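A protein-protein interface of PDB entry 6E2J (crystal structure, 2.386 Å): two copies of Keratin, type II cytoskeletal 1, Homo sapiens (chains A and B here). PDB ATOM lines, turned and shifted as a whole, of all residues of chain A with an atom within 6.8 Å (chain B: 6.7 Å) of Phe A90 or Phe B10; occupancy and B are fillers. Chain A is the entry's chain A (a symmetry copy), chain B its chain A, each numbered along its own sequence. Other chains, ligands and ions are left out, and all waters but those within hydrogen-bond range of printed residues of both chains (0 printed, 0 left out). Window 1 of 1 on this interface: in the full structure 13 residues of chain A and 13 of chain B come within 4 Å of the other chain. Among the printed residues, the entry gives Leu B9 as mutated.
Among the printed residues, merely in contact across the chains: Gln A86 with Leu B14 (3.8 Å), Phe A90 with Tyr B6 (3.9 Å), Phe A90 with Phe B10 (3.5 Å) and Leu A94 with Phe B7 (3.4 Å).
No position is printed for both chains.
Of the 4 pairs that touch across the chains among the printed residues, none has its exchanged pair printed and touching as well.
Hydrophobic or aromatic side chains of chain B that line the printed part of chain A: Phe B7, Phe B10 and Leu B14.
Printed residues of chain A that touch a printed residue of chain B: Gln A86, Phe A90 and Leu A94.
Hydrophobic or aromatic side chains of chain A within 4 Å of the printed part of chain B: Phe A90 and Leu A94.
Among the printed residues, no Asp or Glu carboxylate lies within 4 Å of a Lys or Arg side-chain nitrogen of the other chain.
Printed residues of chain B within 4 Å of Gln A86: Leu B14 (3.8 Å).
Phe A90 touches just these residues of chain B: Tyr B6 and Phe B10.
Of the printed residues of chain B, Leu A94 touches Phe B7.
Pro B5 touches none of the printed residues of chain A.
Of the printed residues of chain A, Tyr B6 touches Phe A90 (3.9 Å).
Of the printed residues of chain A, Phe B7 touches Leu A94 (3.4 Å).
Phe B10 touches just one residue of chain A: Phe A90 (3.5 Å).
Of the printed residues of chain A, Leu B14 touches Gln A86 (3.8 Å).
The nearest printed residue of chain B that does not touch Leu A94 is Tyr B6 (4.1 Å).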
ATOM      1  N   ASN A  83       1.785 -15.908  13.891  1.00  0.00           N
ATOM      2  CA  ASN A  83       1.898 -17.363  13.930  1.00  0.00           C
ATOM      3  C   ASN A  83       3.281 -17.789  14.402  1.00  0.00           C
ATOM      4  O   ASN A  83       3.407 -18.679  15.254  1.00  0.00           O
ATOM      5  CB  ASN A  83       1.593 -17.952  12.555  1.00  0.00           C
ATOM      6  CG  ASN A  83       0.110 -18.145  12.329  1.00  0.00           C
ATOM      7  OD1 ASN A  83      -0.717 -17.626  13.081  1.00  0.00           O
ATOM      8  ND2 ASN A  83      -0.237 -18.897  11.295  1.00  0.00           N
ATOM      9  N   GLN A  85       5.498 -16.168  16.299  1.00  0.00           N
ATOM     10  CA  GLN A  85       5.686 -15.912  17.724  1.00  0.00           C
ATOM     11  C   GLN A  85       4.937 -16.942  18.565  1.00  0.00           C
ATOM     12  O   GLN A  85       5.515 -17.584  19.453  1.00  0.00           O
ATOM     13  CB  GLN A  85       5.219 -14.496  18.071  1.00  0.00           C
ATOM     14  CG  GLN A  85       6.304 -13.578  18.608  1.00  0.00           C
ATOM     15  CD  GLN A  85       7.073 -14.187  19.760  1.00  0.00           C
ATOM     16  OE1 GLN A  85       6.703 -15.238  20.283  1.00  0.00           O
ATOM     17  NE2 GLN A  85       8.154 -13.531  20.156  1.00  0.00           N
ATOM     18  N   GLN A  86       3.641 -17.119  18.285  1.00  0.00           N
ATOM     19  CA  GLN A  86       2.831 -18.063  19.051  1.00  0.00           C
ATOM     20  C   GLN A  86       3.447 -19.456  19.035  1.00  0.00           C
ATOM     21  O   GLN A  86       3.556 -20.111  20.080  1.00  0.00           O
ATOM     22  CB  GLN A  86       1.407 -18.099  18.493  1.00  0.00           C
ATOM     23  CG  GLN A  86       0.672 -16.757  18.574  1.00  0.00           C
ATOM     24  CD  GLN A  86      -0.701 -16.776  17.914  1.00  0.00           C
ATOM     25  OE1 GLN A  86      -1.267 -17.836  17.652  1.00  0.00           O
ATOM     26  NE2 GLN A  86      -1.242 -15.588  17.645  1.00  0.00           N
ATOM     27  N   GLU A  87       3.864 -19.923  17.857  1.00  0.00           N
ATOM     28  CA  GLU A  87       4.453 -21.255  17.768  1.00  0.00           C
ATOM     29  C   GLU A  87       5.770 -21.329  18.533  1.00  0.00           C
ATOM     30  O   GLU A  87       6.045 -22.332  19.199  1.00  0.00           O
ATOM     31  CB  GLU A  87       4.652 -21.652  16.304  1.00  0.00           C
ATOM     32  CG  GLU A  87       5.187 -23.067  16.139  1.00  0.00           C
ATOM     33  CD  GLU A  87       4.924 -23.661  14.765  1.00  0.00           C
ATOM     34  OE1 GLU A  87       4.589 -22.905  13.830  1.00  0.00           O
ATOM     35  OE2 GLU A  87       5.050 -24.896  14.624  1.00  0.00           O
ATOM     36  N   ILE A  88       6.592 -20.280  18.463  1.00  0.00           N
ATOM     37  CA  ILE A  88       7.832 -20.260  19.242  1.00  0.00           C
ATOM     38  C   ILE A  88       7.523 -20.470  20.719  1.00  0.00           C
ATOM     39  O   ILE A  88       8.053 -21.381  21.362  1.00  0.00           O
ATOM     40  CB  ILE A  88       8.604 -18.948  19.017  1.00  0.00           C
ATOM     41  CG1 ILE A  88       9.244 -18.933  17.626  1.00  0.00           C
ATOM     42  CG2 ILE A  88       9.681 -18.788  20.094  1.00  0.00           C
ATOM     43  CD1 ILE A  88      10.035 -17.660  17.294  1.00  0.00           C
ATOM     44  N   ASP A  89       6.660 -19.621  21.282  1.00  0.00           N
ATOM     45  CA  ASP A  89       6.345 -19.728  22.707  1.00  0.00           C
ATOM     46  C   ASP A  89       5.830 -21.122  23.053  1.00  0.00           C
ATOM     47  O   ASP A  89       6.355 -21.795  23.957  1.00  0.00           O
ATOM     48  CB  ASP A  89       5.316 -18.664  23.087  1.00  0.00           C
ATOM     49  CG  ASP A  89       5.846 -17.255  22.920  1.00  0.00           C
ATOM     50  OD1 ASP A  89       7.075 -17.065  23.021  1.00  0.00           O
ATOM     51  OD2 ASP A  89       5.033 -16.335  22.685  1.00  0.00           O
ATOM     52  N   PHE A  90       4.796 -21.572  22.335  1.00  0.00           N
ATOM     53  CA  PHE A  90       4.228 -22.891  22.597  1.00  0.00           C
ATOM     54  C   PHE A  90       5.308 -23.965  22.599  1.00  0.00           C
ATOM     55  O   PHE A  90       5.400 -24.772  23.531  1.00  0.00           O
ATOM     56  CB  PHE A  90       3.159 -23.217  21.556  1.00  0.00           C
ATOM     57  CG  PHE A  90       2.769 -24.667  21.529  1.00  0.00           C
ATOM     58  CD1 PHE A  90       2.036 -25.217  22.567  1.00  0.00           C
ATOM     59  CD2 PHE A  90       3.128 -25.479  20.465  1.00  0.00           C
ATOM     60  CE1 PHE A  90       1.672 -26.549  22.548  1.00  0.00           C
ATOM     61  CE2 PHE A  90       2.766 -26.814  20.440  1.00  0.00           C
ATOM     62  CZ  PHE A  90       2.038 -27.349  21.483  1.00  0.00           C
ATOM     63  N   LEU A  91       6.146 -23.984  21.558  1.00  0.00           N
ATOM     64  CA  LEU A  91       7.183 -25.006  21.449  1.00  0.00           C
ATOM     65  C   LEU A  91       8.208 -24.884  22.568  1.00  0.00           C
ATOM     66  O   LEU A  91       8.765 -25.892  23.010  1.00  0.00           O
ATOM     67  CB  LEU A  91       7.874 -24.912  20.085  1.00  0.00           C
ATOM     68  CG  LEU A  91       7.595 -25.981  19.016  1.00  0.00           C
ATOM     69  CD1 LEU A  91       6.151 -26.478  19.019  1.00  0.00           C
ATOM     70  CD2 LEU A  91       7.946 -25.428  17.632  1.00  0.00           C
ATOM     71  N   THR A  92       8.486 -23.665  23.028  1.00  0.00           N
ATOM     72  CA  THR A  92       9.389 -23.484  24.157  1.00  0.00           C
ATOM     73  C   THR A  92       8.850 -24.198  25.389  1.00  0.00           C
ATOM     74  O   THR A  92       9.495 -25.104  25.942  1.00  0.00           O
ATOM     75  CB  THR A  92       9.575 -21.991  24.434  1.00  0.00           C
ATOM     76  OG1 THR A  92      10.130 -21.353  23.279  1.00  0.00           O
ATOM     77  CG2 THR A  92      10.499 -21.775  25.605  1.00  0.00           C
ATOM     78  N   ALA A  93       7.651 -23.809  25.828  1.00  0.00           N
ATOM     79  CA  ALA A  93       7.056 -24.458  26.992  1.00  0.00           C
ATOM     80  C   ALA A  93       6.994 -25.970  26.799  1.00  0.00           C
ATOM     81  O   ALA A  93       7.459 -26.742  27.650  1.00  0.00           O
ATOM     82  CB  ALA A  93       5.663 -23.881  27.252  1.00  0.00           C
ATOM     83  N   LEU A  94       6.436 -26.412  25.669  1.00  0.00           N
ATOM     84  CA  LEU A  94       6.276 -27.843  25.434  1.00  0.00           C
ATOM     85  C   LEU A  94       7.608 -28.572  25.512  1.00  0.00           C
ATOM     86  O   LEU A  94       7.687 -29.675  26.060  1.00  0.00           O
ATOM     87  CB  LEU A  94       5.629 -28.097  24.073  1.00  0.00           C
ATOM     88  CG  LEU A  94       5.413 -29.585  23.760  1.00  0.00           C
ATOM     89  CD1 LEU A  94       4.435 -30.205  24.751  1.00  0.00           C
ATOM     90  CD2 LEU A  94       4.937 -29.792  22.334  1.00  0.00           C
ATOM     91  N   TYR A  95       8.663 -27.985  24.952  1.00  0.00           N
ATOM     92  CA  TYR A  95       9.940 -28.683  24.910  1.00  0.00           C
ATOM     93  C   TYR A  95      10.566 -28.769  26.296  1.00  0.00           C
ATOM     94  O   TYR A  95      11.063 -29.833  26.685  1.00  0.00           O
ATOM     95  CB  TYR A  95      10.878 -27.998  23.920  1.00  0.00           C
ATOM     96  CG  TYR A  95      10.555 -28.281  22.462  1.00  0.00           C
ATOM     97  CD1 TYR A  95       9.535 -29.159  22.093  1.00  0.00           C
ATOM     98  CD2 TYR A  95      11.281 -27.677  21.457  1.00  0.00           C
ATOM     99  CE1 TYR A  95       9.261 -29.414  20.762  1.00  0.00           C
ATOM    100  CE2 TYR A  95      11.018 -27.926  20.132  1.00  0.00           C
ATOM    101  CZ  TYR A  95      10.010 -28.790  19.787  1.00  0.00           C
ATOM    102  OH  TYR A  95       9.767 -29.010  18.454  1.00  0.00           O
ATOM    103  N   PRO B   5      -2.575 -31.699  27.939  1.00  0.00           N
ATOM    104  CA  PRO B   5      -3.164 -30.367  28.146  1.00  0.00           C
ATOM    105  C   PRO B   5      -2.386 -29.201  27.544  1.00  0.00           C
ATOM    106  O   PRO B   5      -3.000 -28.166  27.263  1.00  0.00           O
ATOM    107  CB  PRO B   5      -3.243 -30.240  29.674  1.00  0.00           C
ATOM    108  CG  PRO B   5      -2.809 -31.548  30.252  1.00  0.00           C
ATOM    109  CD  PRO B   5      -2.704 -32.538  29.147  1.00  0.00           C
ATOM    110  N   TYR B   6      -1.060 -29.286  27.395  1.00  0.00           N
ATOM    111  CA  TYR B   6      -0.357 -28.238  26.655  1.00  0.00           C
ATOM    112  C   TYR B   6      -0.955 -28.094  25.260  1.00  0.00           C
ATOM    113  O   TYR B   6      -1.411 -27.010  24.861  1.00  0.00           O
ATOM    114  CB  TYR B   6       1.143 -28.546  26.556  1.00  0.00           C
ATOM    115  CG  TYR B   6       1.955 -28.164  27.777  1.00  0.00           C
ATOM    116  CD1 TYR B   6       2.325 -26.842  28.009  1.00  0.00           C
ATOM    117  CD2 TYR B   6       2.371 -29.130  28.686  1.00  0.00           C
ATOM    118  CE1 TYR B   6       3.078 -26.493  29.125  1.00  0.00           C
ATOM    119  CE2 TYR B   6       3.120 -28.794  29.796  1.00  0.00           C
ATOM    120  CZ  TYR B   6       3.469 -27.482  30.015  1.00  0.00           C
ATOM    121  OH  TYR B   6       4.209 -27.200  31.136  1.00  0.00           O
ATOM    122  N   PHE B   7      -0.974 -29.198  24.510  1.00  0.00           N
ATOM    123  CA  PHE B   7      -1.570 -29.192  23.179  1.00  0.00           C
ATOM    124  C   PHE B   7      -3.007 -28.693  23.220  1.00  0.00           C
ATOM    125  O   PHE B   7      -3.409 -27.876  22.383  1.00  0.00           O
ATOM    126  CB  PHE B   7      -1.516 -30.594  22.575  1.00  0.00           C
ATOM    127  CG  PHE B   7      -0.144 -31.018  22.132  1.00  0.00           C
ATOM    128  CD1 PHE B   7       0.816 -31.411  23.054  1.00  0.00           C
ATOM    129  CD2 PHE B   7       0.179 -31.034  20.788  1.00  0.00           C
ATOM    130  CE1 PHE B   7       2.077 -31.802  22.635  1.00  0.00           C
ATOM    131  CE2 PHE B   7       1.430 -31.424  20.365  1.00  0.00           C
ATOM    132  CZ  PHE B   7       2.382 -31.809  21.287  1.00  0.00           C
ATOM    133  N   GLU B   8      -3.804 -29.172  24.181  1.00  0.00           N
ATOM    134  CA  GLU B   8      -5.206 -28.762  24.228  1.00  0.00           C
ATOM    135  C   GLU B   8      -5.345 -27.265  24.482  1.00  0.00           C
ATOM    136  O   GLU B   8      -6.254 -26.628  23.937  1.00  0.00           O
ATOM    137  CB  GLU B   8      -5.964 -29.553  25.296  1.00  0.00           C
ATOM    138  CG  GLU B   8      -5.977 -31.063  25.049  1.00  0.00           C
ATOM    139  CD  GLU B   8      -7.103 -31.784  25.770  1.00  0.00           C
ATOM    140  OE1 GLU B   8      -8.235 -31.256  25.797  1.00  0.00           O
ATOM    141  OE2 GLU B   8      -6.856 -32.884  26.309  1.00  0.00           O
ATOM    142  N   LEU B   9      -4.459 -26.688  25.295  1.00  0.00           N
ATOM    143  CA  LEU B   9      -4.497 -25.250  25.539  1.00  0.00           C
ATOM    144  C   LEU B   9      -4.184 -24.486  24.261  1.00  0.00           C
ATOM    145  O   LEU B   9      -4.943 -23.603  23.846  1.00  0.00           O
ATOM    146  CB  LEU B   9      -3.504 -24.881  26.645  1.00  0.00           C
ATOM    147  CG  LEU B   9      -3.646 -23.542  27.385  1.00  0.00           C
ATOM    148  CD1 LEU B   9      -2.268 -23.022  27.758  1.00  0.00           C
ATOM    149  CD2 LEU B   9      -4.399 -22.492  26.598  1.00  0.00           C
ATOM    150  N   PHE B  10      -3.060 -24.811  23.617  1.00  0.00           N
ATOM    151  CA  PHE B  10      -2.704 -24.093  22.399  1.00  0.00           C
ATOM    152  C   PHE B  10      -3.810 -24.212  21.355  1.00  0.00           C
ATOM    153  O   PHE B  10      -4.197 -23.221  20.722  1.00  0.00           O
ATOM    154  CB  PHE B  10      -1.380 -24.616  21.850  1.00  0.00           C
ATOM    155  CG  PHE B  10      -0.874 -23.843  20.676  1.00  0.00           C
ATOM    156  CD1 PHE B  10      -0.568 -22.500  20.804  1.00  0.00           C
ATOM    157  CD2 PHE B  10      -0.694 -24.456  19.451  1.00  0.00           C
ATOM    158  CE1 PHE B  10      -0.101 -21.780  19.731  1.00  0.00           C
ATOM    159  CE2 PHE B  10      -0.225 -23.741  18.371  1.00  0.00           C
ATOM    160  CZ  PHE B  10       0.072 -22.398  18.510  1.00  0.00           C
ATOM    161  N   ILE B  11      -4.342 -25.423  21.173  1.00  0.00           N
ATOM    162  CA  ILE B  11      -5.479 -25.604  20.276  1.00  0.00           C
ATOM    163  C   ILE B  11      -6.627 -24.696  20.689  1.00  0.00           C
ATOM    164  O   ILE B  11      -7.294 -24.095  19.845  1.00  0.00           O
ATOM    165  CB  ILE B  11      -5.921 -27.079  20.247  1.00  0.00           C
ATOM    166  CG1 ILE B  11      -4.843 -27.944  19.588  1.00  0.00           C
ATOM    167  CG2 ILE B  11      -7.252 -27.209  19.508  1.00  0.00           C
ATOM    168  CD1 ILE B  11      -5.240 -29.419  19.364  1.00  0.00           C
ATOM    169  N   ASN B  12      -6.889 -24.595  21.993  1.00  0.00           N
ATOM    170  CA  ASN B  12      -7.988 -23.752  22.450  1.00  0.00           C
ATOM    171  C   ASN B  12      -7.764 -22.304  22.050  1.00  0.00           C
ATOM    172  O   ASN B  12      -8.688 -21.633  21.573  1.00  0.00           O
ATOM    173  CB  ASN B  12      -8.152 -23.871  23.962  1.00  0.00           C
ATOM    174  CG  ASN B  12      -8.969 -25.079  24.359  1.00  0.00           C
ATOM    175  OD1 ASN B  12      -9.728 -25.619  23.555  1.00  0.00           O
ATOM    176  ND2 ASN B  12      -8.819 -25.512  25.603  1.00  0.00           N
ATOM    177  N   ASN B  13      -6.542 -21.806  22.227  1.00  0.00           N
ATOM    178  CA  ASN B  13      -6.231 -20.450  21.794  1.00  0.00           C
ATOM    179  C   ASN B  13      -6.499 -20.289  20.303  1.00  0.00           C
ATOM    180  O   ASN B  13      -7.206 -19.363  19.880  1.00  0.00           O
ATOM    181  CB  ASN B  13      -4.778 -20.122  22.129  1.00  0.00           C
ATOM    182  CG  ASN B  13      -4.523 -20.064  23.623  1.00  0.00           C
ATOM    183  OD1 ASN B  13      -5.438 -20.238  24.430  1.00  0.00           O
ATOM    184  ND2 ASN B  13      -3.272 -19.822  23.999  1.00  0.00           N
ATOM    185  N   LEU B  14      -5.957 -21.200  19.490  1.00  0.00           N
ATOM    186  CA  LEU B  14      -6.173 -21.117  18.048  1.00  0.00           C
ATOM    187  C   LEU B  14      -7.661 -21.129  17.713  1.00  0.00           C
ATOM    188  O   LEU B  14      -8.118 -20.363  16.857  1.00  0.00           O
ATOM    189  CB  LEU B  14      -5.446 -22.265  17.343  1.00  0.00           C
ATOM    190  CG  LEU B  14      -4.041 -21.966  16.801  1.00  0.00           C
ATOM    191  CD1 LEU B  14      -3.201 -21.115  17.751  1.00  0.00           C
ATOM    192  CD2 LEU B  14      -3.309 -23.268  16.496  1.00  0.00           C
ATOM    193  N   ARG B  15      -8.435 -21.980  18.390  1.00  0.00           N
ATOM    194  CA  ARG B  15      -9.873 -22.035  18.155  1.00  0.00           C
ATOM    195  C   ARG B  15     -10.527 -20.702  18.477  1.00  0.00           C
ATOM    196  O   ARG B  15     -11.391 -20.228  17.730  1.00  0.00           O
ATOM    197  CB  ARG B  15     -10.511 -23.140  18.996  1.00  0.00           C
ATOM    198  CG  ARG B  15     -10.253 -24.561  18.526  1.00  0.00           C
ATOM    199  CD  ARG B  15     -11.140 -25.525  19.298  1.00  0.00           C
ATOM    200  NE  ARG B  15     -10.917 -26.929  18.945  1.00  0.00           N
ATOM    201  CZ  ARG B  15     -11.772 -27.705  18.277  1.00  0.00           C
ATOM    202  NH1 ARG B  15     -12.951 -27.245  17.865  1.00  0.00           N
ATOM    203  NH2 ARG B  15     -11.447 -28.964  18.022  1.00  0.00           N
